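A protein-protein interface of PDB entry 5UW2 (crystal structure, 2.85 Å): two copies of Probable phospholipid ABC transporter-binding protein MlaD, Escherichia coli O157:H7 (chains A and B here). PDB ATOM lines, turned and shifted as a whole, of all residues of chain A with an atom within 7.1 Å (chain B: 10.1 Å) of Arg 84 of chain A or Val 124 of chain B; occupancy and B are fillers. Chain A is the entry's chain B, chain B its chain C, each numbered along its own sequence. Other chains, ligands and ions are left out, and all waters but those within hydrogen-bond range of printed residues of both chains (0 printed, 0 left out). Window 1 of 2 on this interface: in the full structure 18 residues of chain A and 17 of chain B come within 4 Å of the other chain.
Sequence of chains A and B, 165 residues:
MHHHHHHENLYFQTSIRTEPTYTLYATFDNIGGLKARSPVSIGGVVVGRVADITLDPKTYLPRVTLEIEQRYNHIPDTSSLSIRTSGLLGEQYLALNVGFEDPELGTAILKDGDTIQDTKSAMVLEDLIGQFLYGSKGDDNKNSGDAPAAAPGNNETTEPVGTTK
The guanidinium group (NH2) of Arg 84 of chain A is in salt-bridge range of the side-chain carboxylate (OD1) of Asp 127 of chain B, at 3.8 Å. N of Thr 85 of chain A sits at hydrogen-bond distance from OE2 of Glu 126 of chain B, at 3.0 Å.
The backbone carbonyl oxygen (O) of Arg 84 of chain A sits at hydrogen-bond distance from the backbone NH (N) of Tyr 93 of chain A, 2.8 Å away.
Among the printed residues, pairs that only touch across the chains: Arg 84 of chain A with Glu 126 of chain B (3.3 Å), Met 123 of chain A with Glu 126 of chain B (3.3 Å), Arg 84 of chain A with Val 124 of chain B (3.7 Å) and Gly 87 of chain A with Leu 125 of chain B (3.8 Å).
No residue of chain B comes within 4 Å of Ile 83 of chain A. Thr 85 of chain A touches one residue of chain B. Printed residues of chain B within 4 Å of Gly 87 of chain A: Leu 125. No residue of chain B comes within 4 Å of Tyr 93 of chain A. Asn 97 of chain A touches none of the printed residues of chain B. Printed residues of chain B within 4 Å of Met 123 of chain A: Glu 126. Asp 29 of chain B touches none of the printed residues of chain A. Val 124 of chain B touches one residue of chain A. Of the printed residues of chain A, Glu 126 of chain B touches Arg 84 (3.3 Å), Thr 85 (3.0 Å) and Met 123 (3.3 Å). Of the printed residues of chain A, Asp 127 of chain B touches Arg 84. The nearest residue of chain B that does not touch Arg 84 of chain A is Asn 30 of chain B (4.4 Å). The nearest residue of chain A that does not touch Val 124 of chain B is Tyr 93 of chain A (5.2 Å). The nearest printed residue of chain A that does not touch Glu 126 of chain B is Ile 83 of chain A (4.2 Å).
Of the 19 printed residues of chain A, 4 touch a printed residue of chain B. Printed residues of chain A that touch a printed residue of chain B: Arg 84, Thr 85, Gly 87 and Met 123. Hydrophobic or aromatic side chains of chain A within 4 Å of the printed part of chain B: Met 123. Of the 20 printed residues of chain B, 4 touch a printed residue of chain A. Among the printed residues, 6 pairs touch across the chains. Among the printed residues, Asp or Glu carboxylates within 4 Å of a Lys or Arg side-chain nitrogen of the other chain: Arg 84 of chain A with Asp 127 of chain B (3.8 Å).
Positions printed for both chains: 83, 85, 120, 121, 122 and 123.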
ATOM      1  N   LEU A  34      -6.941  26.220 -17.488  1.00  0.00           N
ATOM      2  CA  LEU A  34      -7.538  27.003 -18.567  1.00  0.00           C
ATOM      3  C   LEU A  34      -6.997  26.588 -19.927  1.00  0.00           C
ATOM      4  O   LEU A  34      -5.810  26.293 -20.077  1.00  0.00           O
ATOM      5  CB  LEU A  34      -7.285  28.499 -18.366  1.00  0.00           C
ATOM      6  CG  LEU A  34      -8.383  29.393 -17.780  1.00  0.00           C
ATOM      7  CD1 LEU A  34      -7.981  30.848 -17.967  1.00  0.00           C
ATOM      8  CD2 LEU A  34      -9.761  29.142 -18.390  1.00  0.00           C
ATOM      9  N   SER A  82     -11.501  35.788 -12.021  1.00  0.00           N
ATOM     10  CA  SER A  82     -11.010  34.718 -11.154  1.00  0.00           C
ATOM     11  C   SER A  82     -11.155  33.357 -11.827  1.00  0.00           C
ATOM     12  O   SER A  82     -12.242  32.995 -12.274  1.00  0.00           O
ATOM     13  CB  SER A  82     -11.760  34.720  -9.820  1.00  0.00           C
ATOM     14  OG  SER A  82     -11.613  35.960  -9.152  1.00  0.00           O
ATOM     15  N   ILE A  83     -10.062  32.604 -11.894  1.00  0.00           N
ATOM     16  CA  ILE A  83     -10.100  31.254 -12.450  1.00  0.00           C
ATOM     17  C   ILE A  83     -10.642  30.274 -11.415  1.00  0.00           C
ATOM     18  O   ILE A  83     -10.094  30.147 -10.318  1.00  0.00           O
ATOM     19  CB  ILE A  83      -8.708  30.794 -12.927  1.00  0.00           C
ATOM     20  CG1 ILE A  83      -8.201  31.728 -14.028  1.00  0.00           C
ATOM     21  CG2 ILE A  83      -8.765  29.351 -13.434  1.00  0.00           C
ATOM     22  CD1 ILE A  83      -6.774  31.487 -14.442  1.00  0.00           C
ATOM     23  N   ARG A  84     -11.724  29.589 -11.774  1.00  0.00           N
ATOM     24  CA  ARG A  84     -12.400  28.670 -10.863  1.00  0.00           C
ATOM     25  C   ARG A  84     -12.666  27.316 -11.515  1.00  0.00           C
ATOM     26  O   ARG A  84     -12.414  27.134 -12.704  1.00  0.00           O
ATOM     27  CB  ARG A  84     -13.707  29.293 -10.377  1.00  0.00           C
ATOM     28  CG  ARG A  84     -13.488  30.532  -9.530  1.00  0.00           C
ATOM     29  CD  ARG A  84     -14.789  31.232  -9.202  1.00  0.00           C
ATOM     30  NE  ARG A  84     -14.575  32.355  -8.294  1.00  0.00           N
ATOM     31  CZ  ARG A  84     -15.536  33.166  -7.867  1.00  0.00           C
ATOM     32  NH1 ARG A  84     -16.789  32.991  -8.270  1.00  0.00           N
ATOM     33  NH2 ARG A  84     -15.242  34.160  -7.039  1.00  0.00           N
ATOM     34  N   THR A  85     -13.177  26.375 -10.722  1.00  0.00           N
ATOM     35  CA  THR A  85     -13.474  25.024 -11.192  1.00  0.00           C
ATOM     36  C   THR A  85     -14.946  24.668 -10.993  1.00  0.00           C
ATOM     37  O   THR A  85     -15.519  24.932  -9.935  1.00  0.00           O
ATOM     38  CB  THR A  85     -12.606  23.978 -10.460  1.00  0.00           C
ATOM     39  OG1 THR A  85     -11.225  24.346 -10.555  1.00  0.00           O
ATOM     40  CG2 THR A  85     -12.800  22.591 -11.060  1.00  0.00           C
ATOM     41  N   SER A  86     -15.549  24.062 -12.013  1.00  0.00           N
ATOM     42  CA  SER A  86     -16.937  23.619 -11.931  1.00  0.00           C
ATOM     43  C   SER A  86     -17.015  22.337 -11.113  1.00  0.00           C
ATOM     44  O   SER A  86     -16.374  21.343 -11.447  1.00  0.00           O
ATOM     45  CB  SER A  86     -17.523  23.393 -13.326  1.00  0.00           C
ATOM     46  OG  SER A  86     -17.653  24.615 -14.030  1.00  0.00           O
ATOM     47  N   GLY A  87     -17.801  22.360 -10.043  1.00  0.00           N
ATOM     48  CA  GLY A  87     -17.857  21.230  -9.136  1.00  0.00           C
ATOM     49  C   GLY A  87     -16.504  21.050  -8.476  1.00  0.00           C
ATOM     50  O   GLY A  87     -15.777  22.023  -8.276  1.00  0.00           O
ATOM     51  N   GLY A  90     -14.477  19.118 -12.071  1.00  0.00           N
ATOM     52  CA  GLY A  90     -14.831  19.554 -13.409  1.00  0.00           C
ATOM     53  C   GLY A  90     -13.769  20.429 -14.047  1.00  0.00           C
ATOM     54  O   GLY A  90     -12.662  20.565 -13.526  1.00  0.00           O
ATOM     55  N   GLU A  91     -14.115  21.031 -15.179  1.00  0.00           N
ATOM     56  CA  GLU A  91     -13.165  21.829 -15.943  1.00  0.00           C
ATOM     57  C   GLU A  91     -13.039  23.231 -15.360  1.00  0.00           C
ATOM     58  O   GLU A  91     -13.920  23.695 -14.635  1.00  0.00           O
ATOM     59  CB  GLU A  91     -13.582  21.894 -17.412  1.00  0.00           C
ATOM     60  CG  GLU A  91     -13.673  20.529 -18.077  1.00  0.00           C
ATOM     61  CD  GLU A  91     -14.138  20.606 -19.516  1.00  0.00           C
ATOM     62  OE1 GLU A  91     -14.351  21.731 -20.019  1.00  0.00           O
ATOM     63  OE2 GLU A  91     -14.293  19.539 -20.147  1.00  0.00           O
ATOM     64  N   GLN A  92     -11.935  23.895 -15.682  1.00  0.00           N
ATOM     65  CA  GLN A  92     -11.651  25.227 -15.162  1.00  0.00           C
ATOM     66  C   GLN A  92     -12.242  26.302 -16.070  1.00  0.00           C
ATOM     67  O   GLN A  92     -12.269  26.145 -17.292  1.00  0.00           O
ATOM     68  CB  GLN A  92     -10.139  25.427 -15.008  1.00  0.00           C
ATOM     69  CG  GLN A  92      -9.469  24.440 -14.051  1.00  0.00           C
ATOM     70  CD  GLN A  92      -9.356  23.036 -14.623  1.00  0.00           C
ATOM     71  OE1 GLN A  92      -9.820  22.763 -15.729  1.00  0.00           O
ATOM     72  NE2 GLN A  92      -8.739  22.136 -13.865  1.00  0.00           N
ATOM     73  N   TYR A  93     -12.712  27.392 -15.467  1.00  0.00           N
ATOM     74  CA  TYR A  93     -13.337  28.480 -16.214  1.00  0.00           C
ATOM     75  C   TYR A  93     -12.991  29.834 -15.601  1.00  0.00           C
ATOM     76  O   TYR A  93     -12.492  29.905 -14.475  1.00  0.00           O
ATOM     77  CB  TYR A  93     -14.856  28.305 -16.248  1.00  0.00           C
ATOM     78  CG  TYR A  93     -15.528  28.550 -14.913  1.00  0.00           C
ATOM     79  CD1 TYR A  93     -15.622  27.543 -13.963  1.00  0.00           C
ATOM     80  CD2 TYR A  93     -16.079  29.788 -14.610  1.00  0.00           C
ATOM     81  CE1 TYR A  93     -16.236  27.766 -12.744  1.00  0.00           C
ATOM     82  CE2 TYR A  93     -16.696  30.019 -13.396  1.00  0.00           C
ATOM     83  CZ  TYR A  93     -16.773  29.005 -12.467  1.00  0.00           C
ATOM     84  OH  TYR A  93     -17.386  29.232 -11.257  1.00  0.00           O
ATOM     85  N   LEU A  94     -13.266  30.900 -16.351  1.00  0.00           N
ATOM     86  CA  LEU A  94     -13.041  32.266 -15.888  1.00  0.00           C
ATOM     87  C   LEU A  94     -14.319  32.933 -15.390  1.00  0.00           C
ATOM     88  O   LEU A  94     -15.255  33.159 -16.160  1.00  0.00           O
ATOM     89  CB  LEU A  94     -12.438  33.112 -17.009  1.00  0.00           C
ATOM     90  CG  LEU A  94     -10.933  32.969 -17.230  1.00  0.00           C
ATOM     91  CD1 LEU A  94     -10.537  33.670 -18.509  1.00  0.00           C
ATOM     92  CD2 LEU A  94     -10.146  33.535 -16.059  1.00  0.00           C
ATOM     93  N   ALA A  95     -14.347  33.244 -14.099  1.00  0.00           N
ATOM     94  CA  ALA A  95     -15.447  33.997 -13.512  1.00  0.00           C
ATOM     95  C   ALA A  95     -15.149  35.491 -13.570  1.00  0.00           C
ATOM     96  O   ALA A  95     -14.173  35.964 -12.978  1.00  0.00           O
ATOM     97  CB  ALA A  95     -15.686  33.559 -12.077  1.00  0.00           C
ATOM     98  N   LEU A  96     -15.989  36.223 -14.300  1.00  0.00           N
ATOM     99  CA  LEU A  96     -15.865  37.671 -14.423  1.00  0.00           C
ATOM    100  C   LEU A  96     -16.772  38.378 -13.418  1.00  0.00           C
ATOM    101  O   LEU A  96     -17.989  38.430 -13.605  1.00  0.00           O
ATOM    102  CB  LEU A  96     -16.208  38.114 -15.848  1.00  0.00           C
ATOM    103  CG  LEU A  96     -16.107  39.611 -16.155  1.00  0.00           C
ATOM    104  CD1 LEU A  96     -14.669  40.092 -16.078  1.00  0.00           C
ATOM    105  CD2 LEU A  96     -16.690  39.909 -17.524  1.00  0.00           C
ATOM    106  N   ASN A  97     -16.180  38.916 -12.356  1.00  0.00           N
ATOM    107  CA  ASN A  97     -16.938  39.653 -11.351  1.00  0.00           C
ATOM    108  C   ASN A  97     -17.134  41.114 -11.748  1.00  0.00           C
ATOM    109  O   ASN A  97     -16.172  41.882 -11.811  1.00  0.00           O
ATOM    110  CB  ASN A  97     -16.227  39.580  -9.999  1.00  0.00           C
ATOM    111  CG  ASN A  97     -15.860  38.162  -9.610  1.00  0.00           C
ATOM    112  OD1 ASN A  97     -16.677  37.423  -9.056  1.00  0.00           O
ATOM    113  ND2 ASN A  97     -14.624  37.769  -9.901  1.00  0.00           N
ATOM    114  N   LYS A 120      -7.391  37.268 -10.467  1.00  0.00           N
ATOM    115  CA  LYS A 120      -7.042  36.300  -9.431  1.00  0.00           C
ATOM    116  C   LYS A 120      -6.684  34.980 -10.108  1.00  0.00           C
ATOM    117  O   LYS A 120      -7.412  34.502 -10.979  1.00  0.00           O
ATOM    118  CB  LYS A 120      -8.194  36.105  -8.441  1.00  0.00           C
ATOM    119  CG  LYS A 120      -7.861  35.170  -7.284  1.00  0.00           C
ATOM    120  CD  LYS A 120      -9.016  35.052  -6.300  1.00  0.00           C
ATOM    121  CE  LYS A 120      -8.674  34.113  -5.152  1.00  0.00           C
ATOM    122  NZ  LYS A 120      -9.798  33.970  -4.185  1.00  0.00           N
ATOM    123  N   SER A 121      -5.563  34.395  -9.702  1.00  0.00           N
ATOM    124  CA  SER A 121      -5.017  33.230 -10.387  1.00  0.00           C
ATOM    125  C   SER A 121      -5.678  31.921  -9.961  1.00  0.00           C
ATOM    126  O   SER A 121      -6.519  31.893  -9.059  1.00  0.00           O
ATOM    127  CB  SER A 121      -3.510  33.146 -10.143  1.00  0.00           C
ATOM    128  OG  SER A 121      -2.870  32.462 -11.204  1.00  0.00           O
ATOM    129  N   ALA A 122      -5.288  30.836 -10.625  1.00  0.00           N
ATOM    130  CA  ALA A 122      -5.827  29.513 -10.335  1.00  0.00           C
ATOM    131  C   ALA A 122      -5.095  28.884  -9.158  1.00  0.00           C
ATOM    132  O   ALA A 122      -3.868  28.960  -9.067  1.00  0.00           O
ATOM    133  CB  ALA A 122      -5.722  28.619 -11.560  1.00  0.00           C
ATOM    134  N   MET A 123      -5.852  28.263  -8.260  1.00  0.00           N
ATOM    135  CA  MET A 123      -5.275  27.606  -7.094  1.00  0.00           C
ATOM    136  C   MET A 123      -4.442  26.396  -7.502  1.00  0.00           C
ATOM    137  O   MET A 123      -4.702  25.772  -8.530  1.00  0.00           O
ATOM    138  CB  MET A 123      -6.377  27.182  -6.120  1.00  0.00           C
ATOM    139  CG  MET A 123      -7.188  28.344  -5.567  1.00  0.00           C
ATOM    140  SD  MET A 123      -8.454  27.822  -4.394  1.00  0.00           S
ATOM    141  CE  MET A 123      -8.955  29.403  -3.722  1.00  0.00           C
ATOM    142  N   ASP B  29     -27.142  35.711  -7.233  1.00  0.00           N
ATOM    143  CA  ASP B  29     -25.844  36.333  -7.473  1.00  0.00           C
ATOM    144  C   ASP B  29     -24.989  35.386  -8.307  1.00  0.00           C
ATOM    145  O   ASP B  29     -24.160  35.816  -9.110  1.00  0.00           O
ATOM    146  CB  ASP B  29     -25.140  36.669  -6.155  1.00  0.00           C
ATOM    147  CG  ASP B  29     -25.791  37.829  -5.420  1.00  0.00           C
ATOM    148  OD1 ASP B  29     -26.326  38.739  -6.089  1.00  0.00           O
ATOM    149  OD2 ASP B  29     -25.759  37.833  -4.171  1.00  0.00           O
ATOM    150  N   ASN B  30     -25.200  34.090  -8.097  1.00  0.00           N
ATOM    151  CA  ASN B  30     -24.493  33.048  -8.832  1.00  0.00           C
ATOM    152  C   ASN B  30     -25.348  31.790  -8.928  1.00  0.00           C
ATOM    153  O   ASN B  30     -25.800  31.262  -7.910  1.00  0.00           O
ATOM    154  CB  ASN B  30     -23.155  32.728  -8.160  1.00  0.00           C
ATOM    155  CG  ASN B  30     -22.276  31.810  -8.998  1.00  0.00           C
ATOM    156  OD1 ASN B  30     -22.739  30.813  -9.552  1.00  0.00           O
ATOM    157  ND2 ASN B  30     -20.996  32.148  -9.094  1.00  0.00           N
ATOM    158  N   ILE B  31     -25.565  31.310 -10.150  1.00  0.00           N
ATOM    159  CA  ILE B  31     -26.376  30.116 -10.365  1.00  0.00           C
ATOM    160  C   ILE B  31     -25.511  28.858 -10.429  1.00  0.00           C
ATOM    161  O   ILE B  31     -26.016  27.741 -10.319  1.00  0.00           O
ATOM    162  CB  ILE B  31     -27.209  30.215 -11.653  1.00  0.00           C
ATOM    163  CG1 ILE B  31     -26.307  30.456 -12.867  1.00  0.00           C
ATOM    164  CG2 ILE B  31     -28.251  31.316 -11.518  1.00  0.00           C
ATOM    165  CD1 ILE B  31     -26.763  29.723 -14.100  1.00  0.00           C
ATOM    166  N   GLY B  32     -24.207  29.052 -10.609  1.00  0.00           N
ATOM    167  CA  GLY B  32     -23.269  27.945 -10.667  1.00  0.00           C
ATOM    168  C   GLY B  32     -23.496  27.032 -11.855  1.00  0.00           C
ATOM    169  O   GLY B  32     -23.504  27.479 -13.003  1.00  0.00           O
ATOM    170  N   GLY B  33     -23.688  25.746 -11.574  1.00  0.00           N
ATOM    171  CA  GLY B  33     -23.835  24.744 -12.612  1.00  0.00           C
ATOM    172  C   GLY B  33     -25.245  24.637 -13.156  1.00  0.00           C
ATOM    173  O   GLY B  33     -25.521  23.776 -13.992  1.00  0.00           O
ATOM    174  N   ILE B  83     -29.715  26.783  -4.422  1.00  0.00           N
ATOM    175  CA  ILE B  83     -29.032  25.964  -5.414  1.00  0.00           C
ATOM    176  C   ILE B  83     -28.128  24.956  -4.715  1.00  0.00           C
ATOM    177  O   ILE B  83     -27.240  25.330  -3.945  1.00  0.00           O
ATOM    178  CB  ILE B  83     -28.219  26.829  -6.391  1.00  0.00           C
ATOM    179  CG1 ILE B  83     -29.164  27.765  -7.146  1.00  0.00           C
ATOM    180  CG2 ILE B  83     -27.445  25.950  -7.375  1.00  0.00           C
ATOM    181  CD1 ILE B  83     -28.478  28.786  -7.996  1.00  0.00           C
ATOM    182  N   THR B  85     -26.369  20.605  -4.901  1.00  0.00           N
ATOM    183  CA  THR B  85     -25.798  19.565  -5.749  1.00  0.00           C
ATOM    184  C   THR B  85     -26.274  18.190  -5.283  1.00  0.00           C
ATOM    185  O   THR B  85     -26.285  17.903  -4.085  1.00  0.00           O
ATOM    186  CB  THR B  85     -24.257  19.609  -5.731  1.00  0.00           C
ATOM    187  OG1 THR B  85     -23.809  20.936  -6.038  1.00  0.00           O
ATOM    188  CG2 THR B  85     -23.672  18.629  -6.742  1.00  0.00           C
ATOM    189  N   LYS B 120     -30.890  31.642  -2.247  1.00  0.00           N
ATOM    190  CA  LYS B 120     -29.524  31.313  -1.847  1.00  0.00           C
ATOM    191  C   LYS B 120     -28.722  30.863  -3.063  1.00  0.00           C
ATOM    192  O   LYS B 120     -29.181  30.038  -3.854  1.00  0.00           O
ATOM    193  CB  LYS B 120     -29.514  30.225  -0.770  1.00  0.00           C
ATOM    194  CG  LYS B 120     -28.124  29.885  -0.239  1.00  0.00           C
ATOM    195  CD  LYS B 120     -28.190  28.850   0.877  1.00  0.00           C
ATOM    196  CE  LYS B 120     -26.807  28.506   1.413  1.00  0.00           C
ATOM    197  NZ  LYS B 120     -26.869  27.491   2.504  1.00  0.00           N
ATOM    198  N   SER B 121     -27.521  31.410  -3.204  1.00  0.00           N
ATOM    199  CA  SER B 121     -26.707  31.190  -4.393  1.00  0.00           C
ATOM    200  C   SER B 121     -25.950  29.867  -4.334  1.00  0.00           C
ATOM    201  O   SER B 121     -25.998  29.151  -3.334  1.00  0.00           O
ATOM    202  CB  SER B 121     -25.715  32.341  -4.573  1.00  0.00           C
ATOM    203  OG  SER B 121     -25.874  32.946  -5.841  1.00  0.00           O
ATOM    204  N   ALA B 122     -25.252  29.554  -5.421  1.00  0.00           N
ATOM    205  CA  ALA B 122     -24.472  28.326  -5.526  1.00  0.00           C
ATOM    206  C   ALA B 122     -23.105  28.494  -4.869  1.00  0.00           C
ATOM    207  O   ALA B 122     -22.467  29.538  -5.010  1.00  0.00           O
ATOM    208  CB  ALA B 122     -24.313  27.925  -6.986  1.00  0.00           C
ATOM    209  N   MET B 123     -22.662  27.469  -4.145  1.00  0.00           N
ATOM    210  CA  MET B 123     -21.362  27.511  -3.487  1.00  0.00           C
ATOM    211  C   MET B 123     -20.237  27.551  -4.513  1.00  0.00           C
ATOM    212  O   MET B 123     -20.379  27.031  -5.619  1.00  0.00           O
ATOM    213  CB  MET B 123     -21.167  26.293  -2.586  1.00  0.00           C
ATOM    214  CG  MET B 123     -22.173  26.151  -1.460  1.00  0.00           C
ATOM    215  SD  MET B 123     -21.830  24.711  -0.425  1.00  0.00           S
ATOM    216  CE  MET B 123     -21.780  23.391  -1.643  1.00  0.00           C
ATOM    217  N   VAL B 124     -19.123  28.172  -4.134  1.00  0.00           N
ATOM    218  CA  VAL B 124     -17.931  28.220  -4.975  1.00  0.00           C
ATOM    219  C   VAL B 124     -16.772  27.524  -4.267  1.00  0.00           C
ATOM    220  O   VAL B 124     -16.422  27.883  -3.142  1.00  0.00           O
ATOM    221  CB  VAL B 124     -17.540  29.671  -5.320  1.00  0.00           C
ATOM    222  CG1 VAL B 124     -16.321  29.702  -6.239  1.00  0.00           C
ATOM    223  CG2 VAL B 124     -18.717  30.398  -5.960  1.00  0.00           C
ATOM    224  N   LEU B 125     -16.184  26.530  -4.930  1.00  0.00           N
ATOM    225  CA  LEU B 125     -15.105  25.738  -4.347  1.00  0.00           C
ATOM    226  C   LEU B 125     -13.967  26.619  -3.834  1.00  0.00           C
ATOM    227  O   LEU B 125     -13.469  26.422  -2.726  1.00  0.00           O
ATOM    228  CB  LEU B 125     -14.566  24.740  -5.377  1.00  0.00           C
ATOM    229  CG  LEU B 125     -13.426  23.823  -4.919  1.00  0.00           C
ATOM    230  CD1 LEU B 125     -13.880  22.900  -3.799  1.00  0.00           C
ATOM    231  CD2 LEU B 125     -12.884  23.019  -6.093  1.00  0.00           C
ATOM    232  N   GLU B 126     -13.570  27.594  -4.646  1.00  0.00           N
ATOM    233  CA  GLU B 126     -12.469  28.487  -4.296  1.00  0.00           C
ATOM    234  C   GLU B 126     -12.795  29.293  -3.041  1.00  0.00           C
ATOM    235  O   GLU B 126     -11.931  29.520  -2.194  1.00  0.00           O
ATOM    236  CB  GLU B 126     -12.150  29.432  -5.458  1.00  0.00           C
ATOM    237  CG  GLU B 126     -11.452  28.764  -6.639  1.00  0.00           C
ATOM    238  CD  GLU B 126     -12.349  27.797  -7.397  1.00  0.00           C
ATOM    239  OE1 GLU B 126     -13.588  27.903  -7.272  1.00  0.00           O
ATOM    240  OE2 GLU B 126     -11.812  26.927  -8.114  1.00  0.00           O
ATOM    241  N   ASP B 127     -14.049  29.719  -2.926  1.00  0.00           N
ATOM    242  CA  ASP B 127     -14.485  30.493  -1.771  1.00  0.00           C
ATOM    243  C   ASP B 127     -14.573  29.623  -0.521  1.00  0.00           C
ATOM    244  O   ASP B 127     -14.196  30.052   0.570  1.00  0.00           O
ATOM    245  CB  ASP B 127     -15.839  31.146  -2.053  1.00  0.00           C
ATOM    246  CG  ASP B 127     -15.745  32.257  -3.082  1.00  0.00           C
ATOM    247  OD1 ASP B 127     -14.685  32.383  -3.730  1.00  0.00           O
ATOM    248  OD2 ASP B 127     -16.734  33.003  -3.242  1.00  0.00           O
ATOM    249  N   LEU B 128     -15.076  28.402  -0.683  1.00  0.00           N
ATOM    250  CA  LEU B 128     -15.138  27.452   0.421  1.00  0.00           C
ATOM    251  C   LEU B 128     -13.733  27.133   0.921  1.00  0.00           C
ATOM    252  O   LEU B 128     -13.487  27.100   2.126  1.00  0.00           O
ATOM    253  CB  LEU B 128     -15.854  26.170  -0.004  1.00  0.00           C
ATOM    254  CG  LEU B 128     -17.333  26.310  -0.380  1.00  0.00           C
ATOM    255  CD1 LEU B 128     -17.873  24.978  -0.877  1.00  0.00           C
ATOM    256  CD2 LEU B 128     -18.165  26.825   0.786  1.00  0.00           C
ATOM    257  N   ILE B 129     -12.817  26.893  -0.011  1.00  0.00           N
ATOM    258  CA  ILE B 129     -11.422  26.659   0.338  1.00  0.00           C
ATOM    259  C   ILE B 129     -10.842  27.910   0.988  1.00  0.00           C
ATOM    260  O   ILE B 129     -10.101  27.824   1.967  1.00  0.00           O
ATOM    261  CB  ILE B 129     -10.580  26.270  -0.897  1.00  0.00           C
ATOM    262  CG1 ILE B 129     -11.041  24.920  -1.449  1.00  0.00           C
ATOM    263  CG2 ILE B 129      -9.097  26.192  -0.546  1.00  0.00           C
ATOM    264  CD1 ILE B 129     -10.537  24.625  -2.848  1.00  0.00           C
ATOM    265  N   GLY B 130     -11.182  29.069   0.434  1.00  0.00           N
ATOM    266  CA  GLY B 130     -10.754  30.338   0.995  1.00  0.00           C
ATOM    267  C   GLY B 130     -11.240  30.506   2.423  1.00  0.00           C
ATOM    268  O   GLY B 130     -10.528  31.037   3.277  1.00  0.00           O
ATOM    269  N   GLN B 131     -12.461  30.048   2.677  1.00  0.00           N
ATOM    270  CA  GLN B 131     -13.043  30.101   4.012  1.00  0.00           C
ATOM    271  C   GLN B 131     -12.327  29.136   4.952  1.00  0.00           C
ATOM    272  O   GLN B 131     -11.855  29.531   6.018  1.00  0.00           O
ATOM    273  CB  GLN B 131     -14.538  29.770   3.949  1.00  0.00           C
ATOM    274  CG  GLN B 131     -15.247  29.745   5.298  1.00  0.00           C
ATOM    275  CD  GLN B 131     -15.275  31.101   5.973  1.00  0.00           C
ATOM    276  OE1 GLN B 131     -15.096  32.134   5.326  1.00  0.00           O
ATOM    277  NE2 GLN B 131     -15.504  31.105   7.282  1.00  0.00           N
ATOM    278  N   PHE B 132     -12.256  27.872   4.549  1.00  0.00           N
ATOM    279  CA  PHE B 132     -11.646  26.827   5.366  1.00  0.00           C
ATOM    280  C   PHE B 132     -10.185  27.118   5.698  1.00  0.00           C
ATOM    281  O   PHE B 132      -9.758  26.953   6.841  1.00  0.00           O
ATOM    282  CB  PHE B 132     -11.756  25.477   4.653  1.00  0.00           C
ATOM    283  CG  PHE B 132     -10.993  24.371   5.323  1.00  0.00           C
ATOM    284  CD1 PHE B 132     -11.196  24.080   6.662  1.00  0.00           C
ATOM    285  CD2 PHE B 132     -10.081  23.612   4.609  1.00  0.00           C
ATOM    286  CE1 PHE B 132     -10.496  23.060   7.277  1.00  0.00           C
ATOM    287  CE2 PHE B 132      -9.379  22.590   5.219  1.00  0.00           C
ATOM    288  CZ  PHE B 132      -9.588  22.313   6.555  1.00  0.00           C
